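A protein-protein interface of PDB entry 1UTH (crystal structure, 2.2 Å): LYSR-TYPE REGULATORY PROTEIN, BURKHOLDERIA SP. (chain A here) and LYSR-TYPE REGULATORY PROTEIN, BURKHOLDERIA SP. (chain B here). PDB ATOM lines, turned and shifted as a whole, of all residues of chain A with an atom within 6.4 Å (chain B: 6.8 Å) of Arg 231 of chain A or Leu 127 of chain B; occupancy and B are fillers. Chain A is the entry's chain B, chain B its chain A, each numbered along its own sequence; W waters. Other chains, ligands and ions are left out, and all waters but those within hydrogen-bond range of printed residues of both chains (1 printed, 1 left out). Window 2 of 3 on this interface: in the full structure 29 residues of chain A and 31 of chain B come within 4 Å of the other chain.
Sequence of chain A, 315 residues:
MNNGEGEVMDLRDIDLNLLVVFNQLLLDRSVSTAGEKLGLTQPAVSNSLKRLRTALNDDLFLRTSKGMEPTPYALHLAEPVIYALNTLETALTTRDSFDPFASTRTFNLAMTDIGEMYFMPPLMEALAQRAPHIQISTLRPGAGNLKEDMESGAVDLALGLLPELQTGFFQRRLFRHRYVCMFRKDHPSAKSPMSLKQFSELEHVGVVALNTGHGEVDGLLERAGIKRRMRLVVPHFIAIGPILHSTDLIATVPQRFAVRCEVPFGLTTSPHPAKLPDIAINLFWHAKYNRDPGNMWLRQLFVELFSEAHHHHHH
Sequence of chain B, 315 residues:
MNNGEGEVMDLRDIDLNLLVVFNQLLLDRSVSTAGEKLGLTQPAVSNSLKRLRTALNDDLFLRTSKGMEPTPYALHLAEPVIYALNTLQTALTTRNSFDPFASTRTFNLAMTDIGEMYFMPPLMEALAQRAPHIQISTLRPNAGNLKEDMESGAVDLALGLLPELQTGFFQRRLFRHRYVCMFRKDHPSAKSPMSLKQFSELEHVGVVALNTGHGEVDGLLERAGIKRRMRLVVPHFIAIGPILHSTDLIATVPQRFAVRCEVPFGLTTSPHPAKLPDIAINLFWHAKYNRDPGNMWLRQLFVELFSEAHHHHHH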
ATOM      1  N   GLU A 203      21.956  19.633  -9.347  1.00  0.00           N
ATOM      2  CA  GLU A 203      21.784  18.831  -8.112  1.00  0.00           C
ATOM      3  C   GLU A 203      22.383  19.576  -6.917  1.00  0.00           C
ATOM      4  O   GLU A 203      23.346  20.304  -7.076  1.00  0.00           O
ATOM      5  CB  GLU A 203      22.486  17.483  -8.238  1.00  0.00           C
ATOM      6  CG  GLU A 203      22.007  16.606  -9.393  1.00  0.00           C
ATOM      7  CD  GLU A 203      22.593  15.222  -9.291  1.00  0.00           C
ATOM      8  OE1 GLU A 203      23.796  15.075  -9.576  1.00  0.00           O
ATOM      9  OE2 GLU A 203      21.861  14.312  -8.891  1.00  0.00           O
ATOM     10  N   HIS A 204      21.805  19.393  -5.739  1.00  0.00           N
ATOM     11  CA  HIS A 204      22.105  20.261  -4.610  1.00  0.00           C
ATOM     12  C   HIS A 204      22.509  19.458  -3.390  1.00  0.00           C
ATOM     13  O   HIS A 204      22.077  18.312  -3.235  1.00  0.00           O
ATOM     14  CB  HIS A 204      20.881  21.082  -4.179  1.00  0.00           C
ATOM     15  CG  HIS A 204      20.357  22.030  -5.212  1.00  0.00           C
ATOM     16  ND1 HIS A 204      19.989  23.318  -4.909  1.00  0.00           N
ATOM     17  CD2 HIS A 204      20.077  21.865  -6.527  1.00  0.00           C
ATOM     18  CE1 HIS A 204      19.520  23.912  -5.993  1.00  0.00           C
ATOM     19  NE2 HIS A 204      19.565  23.054  -6.990  1.00  0.00           N
ATOM     20  N   VAL A 205      23.314  20.090  -2.523  1.00  0.00           N
ATOM     21  CA  VAL A 205      23.431  19.683  -1.123  1.00  0.00           C
ATOM     22  C   VAL A 205      22.677  20.673  -0.317  1.00  0.00           C
ATOM     23  O   VAL A 205      22.883  21.874  -0.494  1.00  0.00           O
ATOM     24  CB  VAL A 205      24.832  19.924  -0.419  1.00  0.00           C
ATOM     25  CG1 VAL A 205      25.125  18.819   0.575  1.00  0.00           C
ATOM     26  CG2 VAL A 205      25.958  20.281  -1.360  1.00  0.00           C
ATOM     27  N   ARG A 228      13.933  21.433  -6.268  1.00  0.00           N
ATOM     28  CA  ARG A 228      15.352  21.082  -6.060  1.00  0.00           C
ATOM     29  C   ARG A 228      15.530  19.588  -5.946  1.00  0.00           C
ATOM     30  O   ARG A 228      14.887  18.938  -5.116  1.00  0.00           O
ATOM     31  CB  ARG A 228      15.896  21.755  -4.798  1.00  0.00           C
ATOM     32  CG  ARG A 228      16.519  23.113  -5.054  1.00  0.00           C
ATOM     33  CD  ARG A 228      17.123  23.743  -3.808  1.00  0.00           C
ATOM     34  NE  ARG A 228      16.265  23.499  -2.659  1.00  0.00           N
ATOM     35  CZ  ARG A 228      16.648  23.512  -1.397  1.00  0.00           C
ATOM     36  NH1 ARG A 228      17.908  23.811  -1.034  1.00  0.00           N
ATOM     37  NH2 ARG A 228      15.731  23.241  -0.482  1.00  0.00           N
ATOM     38  N   ARG A 229      16.419  19.055  -6.769  1.00  0.00           N
ATOM     39  CA  ARG A 229      16.849  17.667  -6.624  1.00  0.00           C
ATOM     40  C   ARG A 229      17.848  17.598  -5.443  1.00  0.00           C
ATOM     41  O   ARG A 229      18.993  18.002  -5.562  1.00  0.00           O
ATOM     42  CB  ARG A 229      17.502  17.154  -7.925  1.00  0.00           C
ATOM     43  CG  ARG A 229      16.764  17.489  -9.237  1.00  0.00           C
ATOM     44  CD  ARG A 229      17.661  17.473 -10.498  1.00  0.00           C
ATOM     45  NE  ARG A 229      18.002  16.102 -10.922  1.00  0.00           N
ATOM     46  CZ  ARG A 229      19.046  15.764 -11.691  1.00  0.00           C
ATOM     47  NH1 ARG A 229      19.895  16.673 -12.158  1.00  0.00           N
ATOM     48  NH2 ARG A 229      19.241  14.491 -11.995  1.00  0.00           N
ATOM     49  N   MET A 230      17.403  17.123  -4.299  1.00  0.00           N
ATOM     50  CA  MET A 230      18.258  17.092  -3.116  1.00  0.00           C
ATOM     51  C   MET A 230      19.083  15.812  -3.059  1.00  0.00           C
ATOM     52  O   MET A 230      18.744  14.867  -2.364  1.00  0.00           O
ATOM     53  CB  MET A 230      17.407  17.223  -1.843  1.00  0.00           C
ATOM     54  CG  MET A 230      16.558  18.477  -1.802  1.00  0.00           C
ATOM     55  SD  MET A 230      17.494  20.015  -1.970  1.00  0.00           S
ATOM     56  CE  MET A 230      18.417  19.961  -0.517  1.00  0.00           C
ATOM     57  N   ARG A 231      20.203  15.815  -3.755  1.00  0.00           N
ATOM     58  CA  ARG A 231      21.094  14.664  -3.777  1.00  0.00           C
ATOM     59  C   ARG A 231      21.667  14.297  -2.402  1.00  0.00           C
ATOM     60  O   ARG A 231      21.739  13.111  -2.046  1.00  0.00           O
ATOM     61  CB  ARG A 231      22.210  14.938  -4.768  1.00  0.00           C
ATOM     62  CG  ARG A 231      23.166  13.810  -4.934  1.00  0.00           C
ATOM     63  CD  ARG A 231      22.621  12.635  -5.696  1.00  0.00           C
ATOM     64  NE  ARG A 231      23.714  11.961  -6.416  1.00  0.00           N
ATOM     65  CZ  ARG A 231      23.920  10.645  -6.456  1.00  0.00           C
ATOM     66  NH1 ARG A 231      23.142   9.770  -5.810  1.00  0.00           N
ATOM     67  NH2 ARG A 231      24.931  10.201  -7.156  1.00  0.00           N
ATOM     68  N   LEU A 232      22.044  15.311  -1.625  1.00  0.00           N
ATOM     69  CA  LEU A 232      22.498  15.105  -0.237  1.00  0.00           C
ATOM     70  C   LEU A 232      21.897  16.127   0.725  1.00  0.00           C
ATOM     71  O   LEU A 232      21.816  17.300   0.401  1.00  0.00           O
ATOM     72  CB  LEU A 232      24.023  15.293  -0.187  1.00  0.00           C
ATOM     73  CG  LEU A 232      24.952  14.608   0.824  1.00  0.00           C
ATOM     74  CD1 LEU A 232      26.168  15.539   1.117  1.00  0.00           C
ATOM     75  CD2 LEU A 232      24.324  14.099   2.090  1.00  0.00           C
ATOM     76  N   VAL A 233      21.555  15.686   1.934  1.00  0.00           N
ATOM     77  CA  VAL A 233      21.158  16.582   2.983  1.00  0.00           C
ATOM     78  C   VAL A 233      22.021  16.306   4.210  1.00  0.00           C
ATOM     79  O   VAL A 233      22.096  15.174   4.657  1.00  0.00           O
ATOM     80  CB  VAL A 233      19.634  16.360   3.357  1.00  0.00           C
ATOM     81  CG1 VAL A 233      19.279  17.024   4.698  1.00  0.00           C
ATOM     82  CG2 VAL A 233      18.725  16.894   2.223  1.00  0.00           C
ATOM     83  N   LEU A 249      27.827  19.222  -7.147  1.00  0.00           N
ATOM     84  CA  LEU A 249      26.716  19.729  -6.364  1.00  0.00           C
ATOM     85  C   LEU A 249      26.801  21.236  -6.177  1.00  0.00           C
ATOM     86  O   LEU A 249      27.876  21.833  -6.252  1.00  0.00           O
ATOM     87  CB  LEU A 249      26.723  19.073  -4.986  1.00  0.00           C
ATOM     88  CG  LEU A 249      25.950  17.795  -4.680  1.00  0.00           C
ATOM     89  CD1 LEU A 249      25.522  17.020  -5.923  1.00  0.00           C
ATOM     90  CD2 LEU A 249      26.685  16.934  -3.684  1.00  0.00           C
ATOM     91  N   MET B 120      31.945  11.928   3.451  1.00  0.00           N
ATOM     92  CA  MET B 120      31.012  12.395   2.437  1.00  0.00           C
ATOM     93  C   MET B 120      31.599  12.859   1.106  1.00  0.00           C
ATOM     94  O   MET B 120      31.027  12.533   0.072  1.00  0.00           O
ATOM     95  CB  MET B 120      30.080  13.481   2.998  1.00  0.00           C
ATOM     96  CG  MET B 120      29.043  12.961   4.021  1.00  0.00           C
ATOM     97  SD  MET B 120      28.237  11.377   3.670  1.00  0.00           S
ATOM     98  CE  MET B 120      27.599  11.752   2.195  1.00  0.00           C
ATOM     99  N   PRO B 122      34.334  11.859  -0.780  1.00  0.00           N
ATOM    100  CA  PRO B 122      34.600  10.753  -1.715  1.00  0.00           C
ATOM    101  C   PRO B 122      33.403   9.810  -1.908  1.00  0.00           C
ATOM    102  O   PRO B 122      33.237   9.235  -3.000  1.00  0.00           O
ATOM    103  CB  PRO B 122      35.808  10.033  -1.093  1.00  0.00           C
ATOM    104  CG  PRO B 122      35.801  10.421   0.357  1.00  0.00           C
ATOM    105  CD  PRO B 122      35.047  11.699   0.497  1.00  0.00           C
ATOM    106  N   LEU B 123      32.570   9.636  -0.882  1.00  0.00           N
ATOM    107  CA  LEU B 123      31.328   8.898  -1.080  1.00  0.00           C
ATOM    108  C   LEU B 123      30.486   9.524  -2.200  1.00  0.00           C
ATOM    109  O   LEU B 123      30.064   8.816  -3.106  1.00  0.00           O
ATOM    110  CB  LEU B 123      30.483   8.811   0.192  1.00  0.00           C
ATOM    111  CG  LEU B 123      29.130   8.091   0.036  1.00  0.00           C
ATOM    112  CD1 LEU B 123      29.371   6.675  -0.422  1.00  0.00           C
ATOM    113  CD2 LEU B 123      28.281   8.067   1.320  1.00  0.00           C
ATOM    114  N   MET B 124      30.259  10.830  -2.156  1.00  0.00           N
ATOM    115  CA  MET B 124      29.390  11.464  -3.147  1.00  0.00           C
ATOM    116  C   MET B 124      30.039  11.411  -4.513  1.00  0.00           C
ATOM    117  O   MET B 124      29.344  11.265  -5.534  1.00  0.00           O
ATOM    118  CB  MET B 124      29.051  12.922  -2.798  1.00  0.00           C
ATOM    119  CG  MET B 124      28.137  13.090  -1.598  1.00  0.00           C
ATOM    120  SD  MET B 124      26.746  11.933  -1.417  1.00  0.00           S
ATOM    121  CE  MET B 124      25.769  12.509  -2.809  1.00  0.00           C
ATOM    122  N   GLU B 125      31.367  11.532  -4.534  1.00  0.00           N
ATOM    123  CA  GLU B 125      32.117  11.440  -5.786  1.00  0.00           C
ATOM    124  C   GLU B 125      31.896  10.082  -6.457  1.00  0.00           C
ATOM    125  O   GLU B 125      31.671  10.015  -7.669  1.00  0.00           O
ATOM    126  CB  GLU B 125      33.611  11.644  -5.539  1.00  0.00           C
ATOM    127  CG  GLU B 125      34.444  11.725  -6.800  1.00  0.00           C
ATOM    128  CD  GLU B 125      35.932  11.843  -6.487  1.00  0.00           C
ATOM    129  OE1 GLU B 125      36.587  12.744  -7.071  1.00  0.00           O
ATOM    130  OE2 GLU B 125      36.428  11.039  -5.638  1.00  0.00           O
ATOM    131  N   ALA B 126      31.929   9.018  -5.658  1.00  0.00           N
ATOM    132  CA  ALA B 126      31.694   7.663  -6.160  1.00  0.00           C
ATOM    133  C   ALA B 126      30.242   7.455  -6.602  1.00  0.00           C
ATOM    134  O   ALA B 126      29.998   6.897  -7.660  1.00  0.00           O
ATOM    135  CB  ALA B 126      32.091   6.599  -5.114  1.00  0.00           C
ATOM    136  N   LEU B 127      29.286   7.927  -5.802  1.00  0.00           N
ATOM    137  CA  LEU B 127      27.876   7.764  -6.133  1.00  0.00           C
ATOM    138  C   LEU B 127      27.472   8.425  -7.453  1.00  0.00           C
ATOM    139  O   LEU B 127      26.555   7.965  -8.109  1.00  0.00           O
ATOM    140  CB  LEU B 127      26.993   8.259  -4.997  1.00  0.00           C
ATOM    141  CG  LEU B 127      27.075   7.437  -3.699  1.00  0.00           C
ATOM    142  CD1 LEU B 127      26.296   8.122  -2.568  1.00  0.00           C
ATOM    143  CD2 LEU B 127      26.593   5.982  -3.867  1.00  0.00           C
ATOM    144  N   ALA B 128      28.152   9.477  -7.863  1.00  0.00           N
ATOM    145  CA  ALA B 128      27.718  10.229  -9.044  1.00  0.00           C
ATOM    146  C   ALA B 128      27.754   9.343 -10.285  1.00  0.00           C
ATOM    147  O   ALA B 128      26.947   9.511 -11.197  1.00  0.00           O
ATOM    148  CB  ALA B 128      28.579  11.473  -9.244  1.00  0.00           C
ATOM    149  N   GLN B 129      28.696   8.400 -10.292  1.00  0.00           N
ATOM    150  CA  GLN B 129      28.929   7.493 -11.417  1.00  0.00           C
ATOM    151  C   GLN B 129      28.168   6.195 -11.252  1.00  0.00           C
ATOM    152  O   GLN B 129      27.596   5.674 -12.219  1.00  0.00           O
ATOM    153  CB  GLN B 129      30.423   7.154 -11.496  1.00  0.00           C
ATOM    154  CG  GLN B 129      31.368   8.368 -11.506  1.00  0.00           C
ATOM    155  CD  GLN B 129      31.229   9.173 -12.784  1.00  0.00           C
ATOM    156  OE1 GLN B 129      31.055   8.599 -13.879  1.00  0.00           O
ATOM    157  NE2 GLN B 129      31.288  10.504 -12.659  1.00  0.00           N
ATOM    158  N   ARG B 130      28.170   5.690 -10.020  1.00  0.00           N
ATOM    159  CA  ARG B 130      27.666   4.376  -9.702  1.00  0.00           C
ATOM    160  C   ARG B 130      26.185   4.274  -9.343  1.00  0.00           C
ATOM    161  O   ARG B 130      25.590   3.227  -9.574  1.00  0.00           O
ATOM    162  CB  ARG B 130      28.463   3.808  -8.535  1.00  0.00           C
ATOM    163  CG  ARG B 130      29.901   3.537  -8.855  1.00  0.00           C
ATOM    164  CD  ARG B 130      30.523   2.567  -7.869  1.00  0.00           C
ATOM    165  NE  ARG B 130      31.919   2.870  -7.576  1.00  0.00           N
ATOM    166  CZ  ARG B 130      32.738   2.037  -6.943  1.00  0.00           C
ATOM    167  NH1 ARG B 130      32.318   0.852  -6.496  1.00  0.00           N
ATOM    168  NH2 ARG B 130      33.981   2.410  -6.735  1.00  0.00           N
ATOM    169  N   ALA B 131      25.608   5.309  -8.728  1.00  0.00           N
ATOM    170  CA  ALA B 131      24.176   5.324  -8.405  1.00  0.00           C
ATOM    171  C   ALA B 131      23.611   6.731  -8.471  1.00  0.00           C
ATOM    172  O   ALA B 131      23.243   7.295  -7.455  1.00  0.00           O
ATOM    173  CB  ALA B 131      23.939   4.722  -7.035  1.00  0.00           C
ATOM    174  N   PRO B 132      23.518   7.300  -9.664  1.00  0.00           N
ATOM    175  CA  PRO B 132      23.232   8.740  -9.824  1.00  0.00           C
ATOM    176  C   PRO B 132      21.843   9.237  -9.391  1.00  0.00           C
ATOM    177  O   PRO B 132      21.644  10.466  -9.370  1.00  0.00           O
ATOM    178  CB  PRO B 132      23.410   8.994 -11.329  1.00  0.00           C
ATOM    179  CG  PRO B 132      23.449   7.632 -11.989  1.00  0.00           C
ATOM    180  CD  PRO B 132      23.667   6.600 -10.945  1.00  0.00           C
ATOM    181  N   HIS B 133      20.916   8.338  -9.067  1.00  0.00           N
ATOM    182  CA  HIS B 133      19.544   8.722  -8.725  1.00  0.00           C
ATOM    183  C   HIS B 133      19.216   8.437  -7.267  1.00  0.00           C
ATOM    184  O   HIS B 133      18.142   8.808  -6.831  1.00  0.00           O
ATOM    185  CB  HIS B 133      18.520   7.990  -9.634  1.00  0.00           C
ATOM    186  CG  HIS B 133      18.852   8.031 -11.099  1.00  0.00           C
ATOM    187  ND1 HIS B 133      18.321   8.967 -11.962  1.00  0.00           N
ATOM    188  CD2 HIS B 133      19.669   7.254 -11.853  1.00  0.00           C
ATOM    189  CE1 HIS B 133      18.799   8.769 -13.181  1.00  0.00           C
ATOM    190  NE2 HIS B 133      19.624   7.738 -13.142  1.00  0.00           N
ATOM    191  N   ILE B 134      20.100   7.779  -6.500  1.00  0.00           N
ATOM    192  CA  ILE B 134      19.845   7.647  -5.061  1.00  0.00           C
ATOM    193  C   ILE B 134      20.037   8.990  -4.324  1.00  0.00           C
ATOM    194  O   ILE B 134      20.580   9.947  -4.855  1.00  0.00           O
ATOM    195  CB  ILE B 134      20.676   6.519  -4.353  1.00  0.00           C
ATOM    196  CG1 ILE B 134      22.142   6.905  -4.203  1.00  0.00           C
ATOM    197  CG2 ILE B 134      20.518   5.155  -5.058  1.00  0.00           C
ATOM    198  CD1 ILE B 134      22.861   6.073  -3.153  1.00  0.00           C
ATOM    199  N   GLN B 135      19.536   9.046  -3.105  1.00  0.00           N
ATOM    200  CA  GLN B 135      19.652  10.229  -2.281  1.00  0.00           C
ATOM    201  C   GLN B 135      20.265   9.812  -0.982  1.00  0.00           C
ATOM    202  O   GLN B 135      19.983   8.709  -0.502  1.00  0.00           O
ATOM    203  CB  GLN B 135      18.279  10.830  -1.990  1.00  0.00           C
ATOM    204  CG  GLN B 135      17.665  11.518  -3.181  1.00  0.00           C
ATOM    205  CD  GLN B 135      16.235  11.930  -2.901  1.00  0.00           C
ATOM    206  OE1 GLN B 135      15.944  13.111  -2.798  1.00  0.00           O
ATOM    207  NE2 GLN B 135      15.362  10.951  -2.712  1.00  0.00           N
ATOM    208  N   ILE B 136      21.046  10.734  -0.409  1.00  0.00           N
ATOM    209  CA  ILE B 136      21.712  10.559   0.885  1.00  0.00           C
ATOM    210  C   ILE B 136      21.348  11.671   1.862  1.00  0.00           C
ATOM    211  O   ILE B 136      21.287  12.834   1.532  1.00  0.00           O
ATOM    212  CB  ILE B 136      23.297  10.547   0.707  1.00  0.00           C
ATOM    213  CG1 ILE B 136      23.737   9.475  -0.309  1.00  0.00           C
ATOM    214  CG2 ILE B 136      23.997  10.359   2.063  1.00  0.00           C
ATOM    215  CD1 ILE B 136      23.502   8.021   0.150  1.00  0.00           C
ATOM    216  N   SER B 137      21.168  11.290   3.101  1.00  0.00           N
ATOM    217  CA  SER B 137      20.859  12.240   4.130  1.00  0.00           C
ATOM    218  C   SER B 137      21.627  11.770   5.337  1.00  0.00           C
ATOM    219  O   SER B 137      21.762  10.558   5.537  1.00  0.00           O
ATOM    220  CB  SER B 137      19.328  12.249   4.374  1.00  0.00           C
ATOM    221  OG  SER B 137      19.015  12.454   5.743  1.00  0.00           O
ATOM    222  N   TRP B 297      24.840  -3.373  -0.428  1.00  0.00           N
ATOM    223  CA  TRP B 297      25.572  -2.678  -1.461  1.00  0.00           C
ATOM    224  C   TRP B 297      26.254  -1.384  -0.958  1.00  0.00           C
ATOM    225  O   TRP B 297      27.366  -1.079  -1.386  1.00  0.00           O
ATOM    226  CB  TRP B 297      24.668  -2.376  -2.645  1.00  0.00           C
ATOM    227  CG  TRP B 297      25.361  -1.636  -3.720  1.00  0.00           C
ATOM    228  CD1 TRP B 297      26.089  -2.161  -4.735  1.00  0.00           C
ATOM    229  CD2 TRP B 297      25.383  -0.219  -3.900  1.00  0.00           C
ATOM    230  NE1 TRP B 297      26.570  -1.156  -5.546  1.00  0.00           N
ATOM    231  CE2 TRP B 297      26.146   0.048  -5.052  1.00  0.00           C
ATOM    232  CE3 TRP B 297      24.831   0.857  -3.199  1.00  0.00           C
ATOM    233  CZ2 TRP B 297      26.386   1.339  -5.508  1.00  0.00           C
ATOM    234  CZ3 TRP B 297      25.057   2.139  -3.656  1.00  0.00           C
ATOM    235  CH2 TRP B 297      25.841   2.370  -4.794  1.00  0.00           C
ATOM    236  N   LEU B 298      25.609  -0.648  -0.051  1.00  0.00           N
ATOM    237  CA  LEU B 298      26.177   0.591   0.468  1.00  0.00           C
ATOM    238  C   LEU B 298      27.334   0.263   1.359  1.00  0.00           C
ATOM    239  O   LEU B 298      28.366   0.903   1.301  1.00  0.00           O
ATOM    240  CB  LEU B 298      25.170   1.419   1.281  1.00  0.00           C
ATOM    241  CG  LEU B 298      25.115   2.951   1.054  1.00  0.00           C
ATOM    242  CD1 LEU B 298      24.401   3.712   2.197  1.00  0.00           C
ATOM    243  CD2 LEU B 298      26.467   3.568   0.705  1.00  0.00           C
ATOM    244  N   LEU B 301      30.413  -0.534  -0.529  1.00  0.00           N
ATOM    245  CA  LEU B 301      31.013   0.678  -1.071  1.00  0.00           C
ATOM    246  C   LEU B 301      31.847   1.388   0.001  1.00  0.00           C
ATOM    247  O   LEU B 301      32.916   1.891  -0.293  1.00  0.00           O
ATOM    248  CB  LEU B 301      29.946   1.648  -1.547  1.00  0.00           C
ATOM    249  CG  LEU B 301      30.139   2.485  -2.802  1.00  0.00           C
ATOM    250  CD1 LEU B 301      29.391   3.811  -2.640  1.00  0.00           C
ATOM    251  CD2 LEU B 301      31.566   2.704  -3.292  1.00  0.00           C
ATOM    252  N   LEU B 305      35.895   2.010  -0.305  1.00  0.00           N
ATOM    253  CA  LEU B 305      36.491   3.349  -0.278  1.00  0.00           C
ATOM    254  C   LEU B 305      37.345   3.624   0.945  1.00  0.00           C
ATOM    255  O   LEU B 305      38.301   4.373   0.861  1.00  0.00           O
ATOM    256  CB  LEU B 305      35.409   4.412  -0.323  1.00  0.00           C
ATOM    257  CG  LEU B 305      34.517   4.415  -1.566  1.00  0.00           C
ATOM    258  CD1 LEU B 305      33.360   5.350  -1.319  1.00  0.00           C
ATOM    259  CD2 LEU B 305      35.342   4.794  -2.838  1.00  0.00           C
HETATM  260  O   HOH W   1      18.869  13.686   0.208  1.00  0.00           O
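The backbone NH (N) of Ile 136 of chain B sits at hydrogen-bond distance from the backbone carbonyl oxygen (O) of Arg 231 of chain A (3.0 Å). OE1 of Gln 135 of chain B sits close to O of Met 230 of chain A, at 3.3 Å. O of Leu 127 of chain B lies within hydrogen-bond range of NH2 of Arg 231 of chain A (2.9 Å). The backbone carbonyl oxygen (O) of Ile 134 of chain B lies within hydrogen-bond range of the guanidinium group (NH1) of Arg 231 of chain A (2.7 Å). The backbone NH of Ala 128 of chain B sits close to the guanidinium group of Arg 231 of chain A. O of Ala 131 of chain B sits at hydrogen-bond distance from NH1 of Arg 231 of chain A, 3.0 Å away. The backbone carbonyl oxygen of Ile 136 of chain B lies within hydrogen-bond range of the backbone NH of Val 233 of chain A, at 2.9 Å.
The side-chain carboxylate (OE2) of Glu 203 of chain A is in salt-bridge range of the guanidinium group (NE) of Arg 231 of chain A (3.9 Å). The backbone carbonyl oxygen of His 204 of chain A sits at hydrogen-bond distance from the backbone NH of Arg 231 of chain A (3.2 Å). The backbone NH (N) of Leu 232 of chain A sits at hydrogen-bond distance from the backbone carbonyl oxygen (O) of His 204 of chain A (3.4 Å). NE of Arg 228 of chain A lies close to SD of Met 230 of chain A, at 3.8 Å.
Glu 203 of chain A touches Pro 132 of chain B (OE2 to O, 3.9 Å). CE of Met 124 of chain B touches CG of Arg 231 of chain A, 3.6 Å away. Arg 231 of chain A touches Pro 132 of chain B (NH2 to CA, 3.5 Å). Arg 231 of chain A touches Gln 135 of chain B. CG of Leu 232 of chain A touches SD of Met 124 of chain B, 3.9 Å away. Leu 232 of chain A touches Ile 136 of chain B. Val 233 of chain A touches Ser 137 of chain B (O to CA, 3.2 Å).
Arg 231 of chain A touches just these residues of chain B: Met 124, Leu 127, Ala 128, Ala 131, Pro 132, Ile 134, Gln 135 and Ile 136. Of the printed residues of chain B, Val 233 of chain A touches Ile 136 and Ser 137. Leu 249 of chain A touches none of the printed residues of chain B. Of chain A, only Arg 231 (2.9 Å) comes within 4 Å of Leu 127 of chain B. Of the printed residues of chain A, Ala 128 of chain B touches Arg 231. Of the printed residues of chain A, Ile 136 of chain B touches Arg 231 (3.0 Å), Leu 232 (3.1 Å) and Val 233 (2.9 Å).
Printed residues of chain A that touch a printed residue of chain B: Glu 203, Met 230, Arg 231, Leu 232 and Val 233. Hydrophobic or aromatic side chains of chain A within 4 Å of the printed part of chain B: Leu 232. Along chain A the printed residues that touch a printed residue of chain B span positions 203 to 233. Of the 21 printed residues of chain B, 9 touch a printed residue of chain A. Hydrophobic or aromatic side chains of chain B within 4 Å of the printed part of chain A: Met 124, Leu 127, Ile 134 and Ile 136.
Water W1 lies within hydrogen-bond range of the backbone carbonyl oxygen (O) of Met 230 of chain A (2.8 Å) and the backbone carbonyl oxygen (O) of Ile 136 of chain B (2.9 Å).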
